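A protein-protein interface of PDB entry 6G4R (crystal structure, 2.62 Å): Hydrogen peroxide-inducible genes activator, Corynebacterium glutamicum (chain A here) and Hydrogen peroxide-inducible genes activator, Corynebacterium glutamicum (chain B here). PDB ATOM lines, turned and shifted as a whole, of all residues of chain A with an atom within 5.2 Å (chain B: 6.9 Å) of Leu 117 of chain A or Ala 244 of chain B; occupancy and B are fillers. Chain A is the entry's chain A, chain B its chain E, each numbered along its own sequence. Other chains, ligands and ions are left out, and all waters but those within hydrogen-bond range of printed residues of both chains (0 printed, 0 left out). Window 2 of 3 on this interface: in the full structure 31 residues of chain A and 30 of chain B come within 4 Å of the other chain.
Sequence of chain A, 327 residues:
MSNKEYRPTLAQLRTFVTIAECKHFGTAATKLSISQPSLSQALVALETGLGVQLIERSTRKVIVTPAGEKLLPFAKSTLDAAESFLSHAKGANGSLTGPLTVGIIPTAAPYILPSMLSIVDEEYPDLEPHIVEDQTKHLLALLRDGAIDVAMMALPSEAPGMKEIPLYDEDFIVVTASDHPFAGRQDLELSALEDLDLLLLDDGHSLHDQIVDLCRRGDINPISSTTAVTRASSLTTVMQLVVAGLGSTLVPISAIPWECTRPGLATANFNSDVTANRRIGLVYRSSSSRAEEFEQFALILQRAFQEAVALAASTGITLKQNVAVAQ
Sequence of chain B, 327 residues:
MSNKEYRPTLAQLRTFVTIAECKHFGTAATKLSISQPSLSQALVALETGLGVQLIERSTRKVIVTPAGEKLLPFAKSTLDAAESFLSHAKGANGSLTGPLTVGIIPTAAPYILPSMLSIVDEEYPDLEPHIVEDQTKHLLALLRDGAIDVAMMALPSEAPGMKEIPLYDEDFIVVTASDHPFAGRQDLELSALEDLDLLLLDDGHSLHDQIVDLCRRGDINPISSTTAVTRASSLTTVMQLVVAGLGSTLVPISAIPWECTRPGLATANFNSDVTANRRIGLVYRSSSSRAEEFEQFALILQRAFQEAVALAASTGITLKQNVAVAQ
OG of Ser 118 of chain A lies within hydrogen-bond range of O of Pro 114 of chain A (3.3 Å).
The backbone carbonyl oxygen (O) of Leu 241 of chain B lies within hydrogen-bond range of the backbone NH (N) of Leu 246 of chain B, at 3.1 Å.
Hydrophobic or aromatic side chains of chain A that line the printed part of chain B: Leu 113, Pro 114 and Leu 117.
Of the 12 printed residues of chain B, 4 touch a printed residue of chain A.
Printed residues of chain B that touch a printed residue of chain A: Gln 240, Leu 241, Ala 244 and Leu 246.
Hydrophobic or aromatic side chains of chain B that line the printed part of chain A: Leu 241, Ala 244 and Leu 246.
Among the printed residues, no Asp or Glu carboxylate lies within 4 Å of a Lys or Arg side-chain nitrogen of the other chain.
Among the printed residues, merely in contact across the chains: Pro 114 of chain A with Gln 240 of chain B (3.2 Å), Leu 113 of chain A with Leu 241 of chain B (3.7 Å), Leu 117 of chain A with Ala 244 of chain B (3.7 Å), Leu 117 of chain A with Leu 241 of chain B (3.7 Å) and Leu 117 of chain A with Leu 246 of chain B (3.9 Å).
Of the printed residues of chain B, Leu 113 of chain A touches Leu 241 (3.7 Å).
Of the printed residues of chain B, Pro 114 of chain A touches Gln 240.
Ser 115 of chain A touches none of the printed residues of chain B.
Of chain B, only Leu 241, Ala 244 and Leu 246 come within 4 Å of Leu 117 of chain A.
Pro 129 of chain A touches none of the printed residues of chain B.
Of the printed residues of chain A, Gln 240 of chain B touches Pro 114.
Printed residues of chain A within 4 Å of Leu 241 of chain B: Leu 113 and Leu 117.
Of chain A, only Leu 117 comes within 4 Å of Ala 244 of chain B.
Printed residues of chain A within 4 Å of Leu 246 of chain B: Leu 117.
The nearest residue of chain B that does not touch Leu 117 of chain A is Gln 240 of chain B (4.4 Å).
The nearest printed residue of chain A that does not touch Leu 246 of chain B is Pro 129 of chain A (4.7 Å).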
ATOM      1  N   ILE A 112       4.055 -13.601 -14.639  1.00  0.00           N
ATOM      2  CA  ILE A 112       3.016 -13.225 -15.590  1.00  0.00           C
ATOM      3  C   ILE A 112       3.094 -11.748 -15.968  1.00  0.00           C
ATOM      4  O   ILE A 112       2.588 -11.367 -17.034  1.00  0.00           O
ATOM      5  CB  ILE A 112       1.616 -13.561 -15.030  1.00  0.00           C
ATOM      6  CG1 ILE A 112       0.595 -13.688 -16.159  1.00  0.00           C
ATOM      7  CG2 ILE A 112       1.165 -12.511 -14.022  1.00  0.00           C
ATOM      8  CD1 ILE A 112       0.685 -14.990 -16.908  1.00  0.00           C
ATOM      9  N   LEU A 113       3.723 -10.910 -15.134  1.00  0.00           N
ATOM     10  CA  LEU A 113       3.746  -9.471 -15.398  1.00  0.00           C
ATOM     11  C   LEU A 113       4.517  -9.097 -16.661  1.00  0.00           C
ATOM     12  O   LEU A 113       4.010  -8.263 -17.433  1.00  0.00           O
ATOM     13  CB  LEU A 113       4.291  -8.732 -14.173  1.00  0.00           C
ATOM     14  CG  LEU A 113       3.299  -8.512 -13.030  1.00  0.00           C
ATOM     15  CD1 LEU A 113       3.954  -7.757 -11.886  1.00  0.00           C
ATOM     16  CD2 LEU A 113       2.069  -7.774 -13.527  1.00  0.00           C
ATOM     17  N   PRO A 114       5.725  -9.622 -16.926  1.00  0.00           N
ATOM     18  CA  PRO A 114       6.469  -9.155 -18.114  1.00  0.00           C
ATOM     19  C   PRO A 114       5.693  -9.258 -19.418  1.00  0.00           C
ATOM     20  O   PRO A 114       5.660  -8.295 -20.195  1.00  0.00           O
ATOM     21  CB  PRO A 114       7.712 -10.056 -18.116  1.00  0.00           C
ATOM     22  CG  PRO A 114       7.893 -10.448 -16.712  1.00  0.00           C
ATOM     23  CD  PRO A 114       6.519 -10.585 -16.140  1.00  0.00           C
ATOM     24  N   SER A 115       5.060 -10.403 -19.677  1.00  0.00           N
ATOM     25  CA  SER A 115       4.267 -10.551 -20.892  1.00  0.00           C
ATOM     26  C   SER A 115       2.949  -9.791 -20.813  1.00  0.00           C
ATOM     27  O   SER A 115       2.483  -9.264 -21.830  1.00  0.00           O
ATOM     28  CB  SER A 115       4.005 -12.031 -21.173  1.00  0.00           C
ATOM     29  OG  SER A 115       3.470 -12.680 -20.032  1.00  0.00           O
ATOM     30  N   MET A 116       2.340  -9.715 -19.628  1.00  0.00           N
ATOM     31  CA  MET A 116       1.063  -9.020 -19.501  1.00  0.00           C
ATOM     32  C   MET A 116       1.235  -7.512 -19.646  1.00  0.00           C
ATOM     33  O   MET A 116       0.434  -6.854 -20.321  1.00  0.00           O
ATOM     34  CB  MET A 116       0.406  -9.365 -18.165  1.00  0.00           C
ATOM     35  CG  MET A 116      -0.999  -8.809 -17.997  1.00  0.00           C
ATOM     36  SD  MET A 116      -1.055  -7.351 -16.937  1.00  0.00           S
ATOM     37  CE  MET A 116      -1.092  -8.116 -15.319  1.00  0.00           C
ATOM     38  N   LEU A 117       2.270  -6.946 -19.020  1.00  0.00           N
ATOM     39  CA  LEU A 117       2.497  -5.508 -19.133  1.00  0.00           C
ATOM     40  C   LEU A 117       2.940  -5.112 -20.535  1.00  0.00           C
ATOM     41  O   LEU A 117       2.658  -3.992 -20.978  1.00  0.00           O
ATOM     42  CB  LEU A 117       3.528  -5.055 -18.100  1.00  0.00           C
ATOM     43  CG  LEU A 117       3.054  -5.071 -16.647  1.00  0.00           C
ATOM     44  CD1 LEU A 117       4.130  -4.528 -15.722  1.00  0.00           C
ATOM     45  CD2 LEU A 117       1.766  -4.277 -16.501  1.00  0.00           C
ATOM     46  N   SER A 118       3.631  -6.005 -21.247  1.00  0.00           N
ATOM     47  CA  SER A 118       4.022  -5.698 -22.619  1.00  0.00           C
ATOM     48  C   SER A 118       2.823  -5.715 -23.558  1.00  0.00           C
ATOM     49  O   SER A 118       2.779  -4.938 -24.518  1.00  0.00           O
ATOM     50  CB  SER A 118       5.086  -6.683 -23.101  1.00  0.00           C
ATOM     51  OG  SER A 118       4.549  -7.987 -23.242  1.00  0.00           O
ATOM     52  N   ILE A 119       1.845  -6.585 -23.297  1.00  0.00           N
ATOM     53  CA  ILE A 119       0.666  -6.654 -24.153  1.00  0.00           C
ATOM     54  C   ILE A 119      -0.206  -5.418 -23.969  1.00  0.00           C
ATOM     55  O   ILE A 119      -0.695  -4.836 -24.945  1.00  0.00           O
ATOM     56  CB  ILE A 119      -0.118  -7.950 -23.878  1.00  0.00           C
ATOM     57  CG1 ILE A 119       0.648  -9.162 -24.410  1.00  0.00           C
ATOM     58  CG2 ILE A 119      -1.506  -7.884 -24.500  1.00  0.00           C
ATOM     59  CD1 ILE A 119       0.025 -10.489 -24.036  1.00  0.00           C
ATOM     60  N   VAL A 120      -0.410  -4.990 -22.720  1.00  0.00           N
ATOM     61  CA  VAL A 120      -1.288  -3.851 -22.473  1.00  0.00           C
ATOM     62  C   VAL A 120      -0.645  -2.553 -22.945  1.00  0.00           C
ATOM     63  O   VAL A 120      -1.348  -1.598 -23.294  1.00  0.00           O
ATOM     64  CB  VAL A 120      -1.679  -3.780 -20.985  1.00  0.00           C
ATOM     65  CG1 VAL A 120      -2.360  -5.069 -20.553  1.00  0.00           C
ATOM     66  CG2 VAL A 120      -0.461  -3.494 -20.117  1.00  0.00           C
ATOM     67  N   ASP A 121       0.687  -2.488 -22.973  1.00  0.00           N
ATOM     68  CA  ASP A 121       1.346  -1.268 -23.427  1.00  0.00           C
ATOM     69  C   ASP A 121       1.203  -1.088 -24.932  1.00  0.00           C
ATOM     70  O   ASP A 121       1.039   0.037 -25.416  1.00  0.00           O
ATOM     71  CB  ASP A 121       2.821  -1.284 -23.028  1.00  0.00           C
ATOM     72  CG  ASP A 121       3.569  -0.054 -23.508  1.00  0.00           C
ATOM     73  OD1 ASP A 121       3.204   1.066 -23.092  1.00  0.00           O
ATOM     74  OD2 ASP A 121       4.519  -0.208 -24.303  1.00  0.00           O
ATOM     75  N   PRO A 129      -2.874   0.149 -15.778  1.00  0.00           N
ATOM     76  CA  PRO A 129      -2.839  -0.940 -14.794  1.00  0.00           C
ATOM     77  C   PRO A 129      -2.032  -0.571 -13.558  1.00  0.00           C
ATOM     78  O   PRO A 129      -0.949   0.014 -13.646  1.00  0.00           O
ATOM     79  CB  PRO A 129      -2.177  -2.086 -15.567  1.00  0.00           C
ATOM     80  CG  PRO A 129      -1.295  -1.401 -16.561  1.00  0.00           C
ATOM     81  CD  PRO A 129      -1.912  -0.058 -16.876  1.00  0.00           C
ATOM     82  N   ILE A 131      -0.745  -2.792 -10.275  1.00  0.00           N
ATOM     83  CA  ILE A 131      -0.598  -4.159  -9.792  1.00  0.00           C
ATOM     84  C   ILE A 131      -0.557  -4.146  -8.272  1.00  0.00           C
ATOM     85  O   ILE A 131       0.125  -3.312  -7.665  1.00  0.00           O
ATOM     86  CB  ILE A 131       0.671  -4.809 -10.374  1.00  0.00           C
ATOM     87  CG1 ILE A 131       0.749  -4.573 -11.883  1.00  0.00           C
ATOM     88  CG2 ILE A 131       0.700  -6.296 -10.059  1.00  0.00           C
ATOM     89  CD1 ILE A 131      -0.417  -5.144 -12.655  1.00  0.00           C
ATOM     90  N   ALA B 177      14.808   1.775 -15.469  1.00  0.00           N
ATOM     91  CA  ALA B 177      14.760   1.153 -16.780  1.00  0.00           C
ATOM     92  C   ALA B 177      15.999   1.535 -17.586  1.00  0.00           C
ATOM     93  O   ALA B 177      16.731   2.469 -17.246  1.00  0.00           O
ATOM     94  CB  ALA B 177      13.490   1.561 -17.526  1.00  0.00           C
ATOM     95  N   MET B 239      10.995  -5.647  -9.767  1.00  0.00           N
ATOM     96  CA  MET B 239      11.912  -5.584 -10.901  1.00  0.00           C
ATOM     97  C   MET B 239      11.167  -5.658 -12.227  1.00  0.00           C
ATOM     98  O   MET B 239      11.496  -4.933 -13.174  1.00  0.00           O
ATOM     99  CB  MET B 239      12.945  -6.704 -10.803  1.00  0.00           C
ATOM    100  CG  MET B 239      13.985  -6.478  -9.728  1.00  0.00           C
ATOM    101  SD  MET B 239      14.606  -4.787  -9.756  1.00  0.00           S
ATOM    102  CE  MET B 239      15.997  -4.934  -8.647  1.00  0.00           C
ATOM    103  N   GLN B 240      10.162  -6.533 -12.320  1.00  0.00           N
ATOM    104  CA  GLN B 240       9.395  -6.634 -13.556  1.00  0.00           C
ATOM    105  C   GLN B 240       8.632  -5.349 -13.845  1.00  0.00           C
ATOM    106  O   GLN B 240       8.419  -5.003 -15.014  1.00  0.00           O
ATOM    107  CB  GLN B 240       8.432  -7.822 -13.488  1.00  0.00           C
ATOM    108  CG  GLN B 240       9.069  -9.141 -13.057  1.00  0.00           C
ATOM    109  CD  GLN B 240       9.997  -9.745 -14.101  1.00  0.00           C
ATOM    110  OE1 GLN B 240      10.343  -9.108 -15.096  1.00  0.00           O
ATOM    111  NE2 GLN B 240      10.399 -10.990 -13.876  1.00  0.00           N
ATOM    112  N   LEU B 241       8.217  -4.627 -12.801  1.00  0.00           N
ATOM    113  CA  LEU B 241       7.561  -3.340 -13.006  1.00  0.00           C
ATOM    114  C   LEU B 241       8.552  -2.290 -13.491  1.00  0.00           C
ATOM    115  O   LEU B 241       8.196  -1.416 -14.291  1.00  0.00           O
ATOM    116  CB  LEU B 241       6.887  -2.882 -11.714  1.00  0.00           C
ATOM    117  CG  LEU B 241       5.874  -3.848 -11.099  1.00  0.00           C
ATOM    118  CD1 LEU B 241       5.276  -3.266  -9.830  1.00  0.00           C
ATOM    119  CD2 LEU B 241       4.788  -4.188 -12.099  1.00  0.00           C
ATOM    120  N   VAL B 242       9.799  -2.357 -13.019  1.00  0.00           N
ATOM    121  CA  VAL B 242      10.807  -1.390 -13.439  1.00  0.00           C
ATOM    122  C   VAL B 242      11.190  -1.617 -14.896  1.00  0.00           C
ATOM    123  O   VAL B 242      11.430  -0.662 -15.646  1.00  0.00           O
ATOM    124  CB  VAL B 242      12.032  -1.457 -12.508  1.00  0.00           C
ATOM    125  CG1 VAL B 242      13.100  -0.476 -12.959  1.00  0.00           C
ATOM    126  CG2 VAL B 242      11.622  -1.168 -11.073  1.00  0.00           C
ATOM    127  N   VAL B 243      11.255  -2.882 -15.322  1.00  0.00           N
ATOM    128  CA  VAL B 243      11.560  -3.183 -16.719  1.00  0.00           C
ATOM    129  C   VAL B 243      10.492  -2.601 -17.636  1.00  0.00           C
ATOM    130  O   VAL B 243      10.797  -2.063 -18.708  1.00  0.00           O
ATOM    131  CB  VAL B 243      11.705  -4.704 -16.918  1.00  0.00           C
ATOM    132  CG1 VAL B 243      11.853  -5.039 -18.394  1.00  0.00           C
ATOM    133  CG2 VAL B 243      12.890  -5.235 -16.127  1.00  0.00           C
ATOM    134  N   ALA B 244       9.228  -2.685 -17.227  1.00  0.00           N
ATOM    135  CA  ALA B 244       8.124  -2.169 -18.025  1.00  0.00           C
ATOM    136  C   ALA B 244       7.991  -0.652 -17.958  1.00  0.00           C
ATOM    137  O   ALA B 244       7.100  -0.096 -18.609  1.00  0.00           O
ATOM    138  CB  ALA B 244       6.814  -2.832 -17.593  1.00  0.00           C
ATOM    139  N   GLY B 245       8.848   0.028 -17.199  1.00  0.00           N
ATOM    140  CA  GLY B 245       8.823   1.477 -17.149  1.00  0.00           C
ATOM    141  C   GLY B 245       7.727   2.097 -16.310  1.00  0.00           C
ATOM    142  O   GLY B 245       7.264   3.196 -16.630  1.00  0.00           O
ATOM    143  N   LEU B 246       7.293   1.425 -15.243  1.00  0.00           N
ATOM    144  CA  LEU B 246       6.301   1.972 -14.326  1.00  0.00           C
ATOM    145  C   LEU B 246       6.933   2.579 -13.078  1.00  0.00           C
ATOM    146  O   LEU B 246       6.249   2.739 -12.062  1.00  0.00           O
ATOM    147  CB  LEU B 246       5.268   0.910 -13.925  1.00  0.00           C
ATOM    148  CG  LEU B 246       4.292   0.235 -14.904  1.00  0.00           C
ATOM    149  CD1 LEU B 246       4.907  -0.229 -16.211  1.00  0.00           C
ATOM    150  CD2 LEU B 246       3.596  -0.930 -14.210  1.00  0.00           C
ATOM    151  N   GLY B 247       8.216   2.919 -13.131  1.00  0.00           N
ATOM    152  CA  GLY B 247       8.895   3.553 -12.023  1.00  0.00           C
ATOM    153  C   GLY B 247      10.232   2.907 -11.735  1.00  0.00           C
ATOM    154  O   GLY B 247      10.640   1.934 -12.366  1.00  0.00           O
ATOM    155  N   GLY B 264      16.668  -5.249 -19.631  1.00  0.00           N
ATOM    156  CA  GLY B 264      15.775  -4.122 -19.472  1.00  0.00           C
ATOM    157  C   GLY B 264      16.024  -3.261 -18.254  1.00  0.00           C
ATOM    158  O   GLY B 264      15.296  -2.282 -18.053  1.00  0.00           O
ATOM    159  N   LEU B 265      17.022  -3.588 -17.439  1.00  0.00           N
ATOM    160  CA  LEU B 265      17.315  -2.842 -16.226  1.00  0.00           C
ATOM    161  C   LEU B 265      18.597  -2.036 -16.380  1.00  0.00           C
ATOM    162  O   LEU B 265      19.402  -2.262 -17.289  1.00  0.00           O
ATOM    163  CB  LEU B 265      17.435  -3.781 -15.019  1.00  0.00           C
ATOM    164  CG  LEU B 265      16.129  -4.363 -14.477  1.00  0.00           C
ATOM    165  CD1 LEU B 265      16.396  -5.261 -13.280  1.00  0.00           C
ATOM    166  CD2 LEU B 265      15.170  -3.245 -14.107  1.00  0.00           C
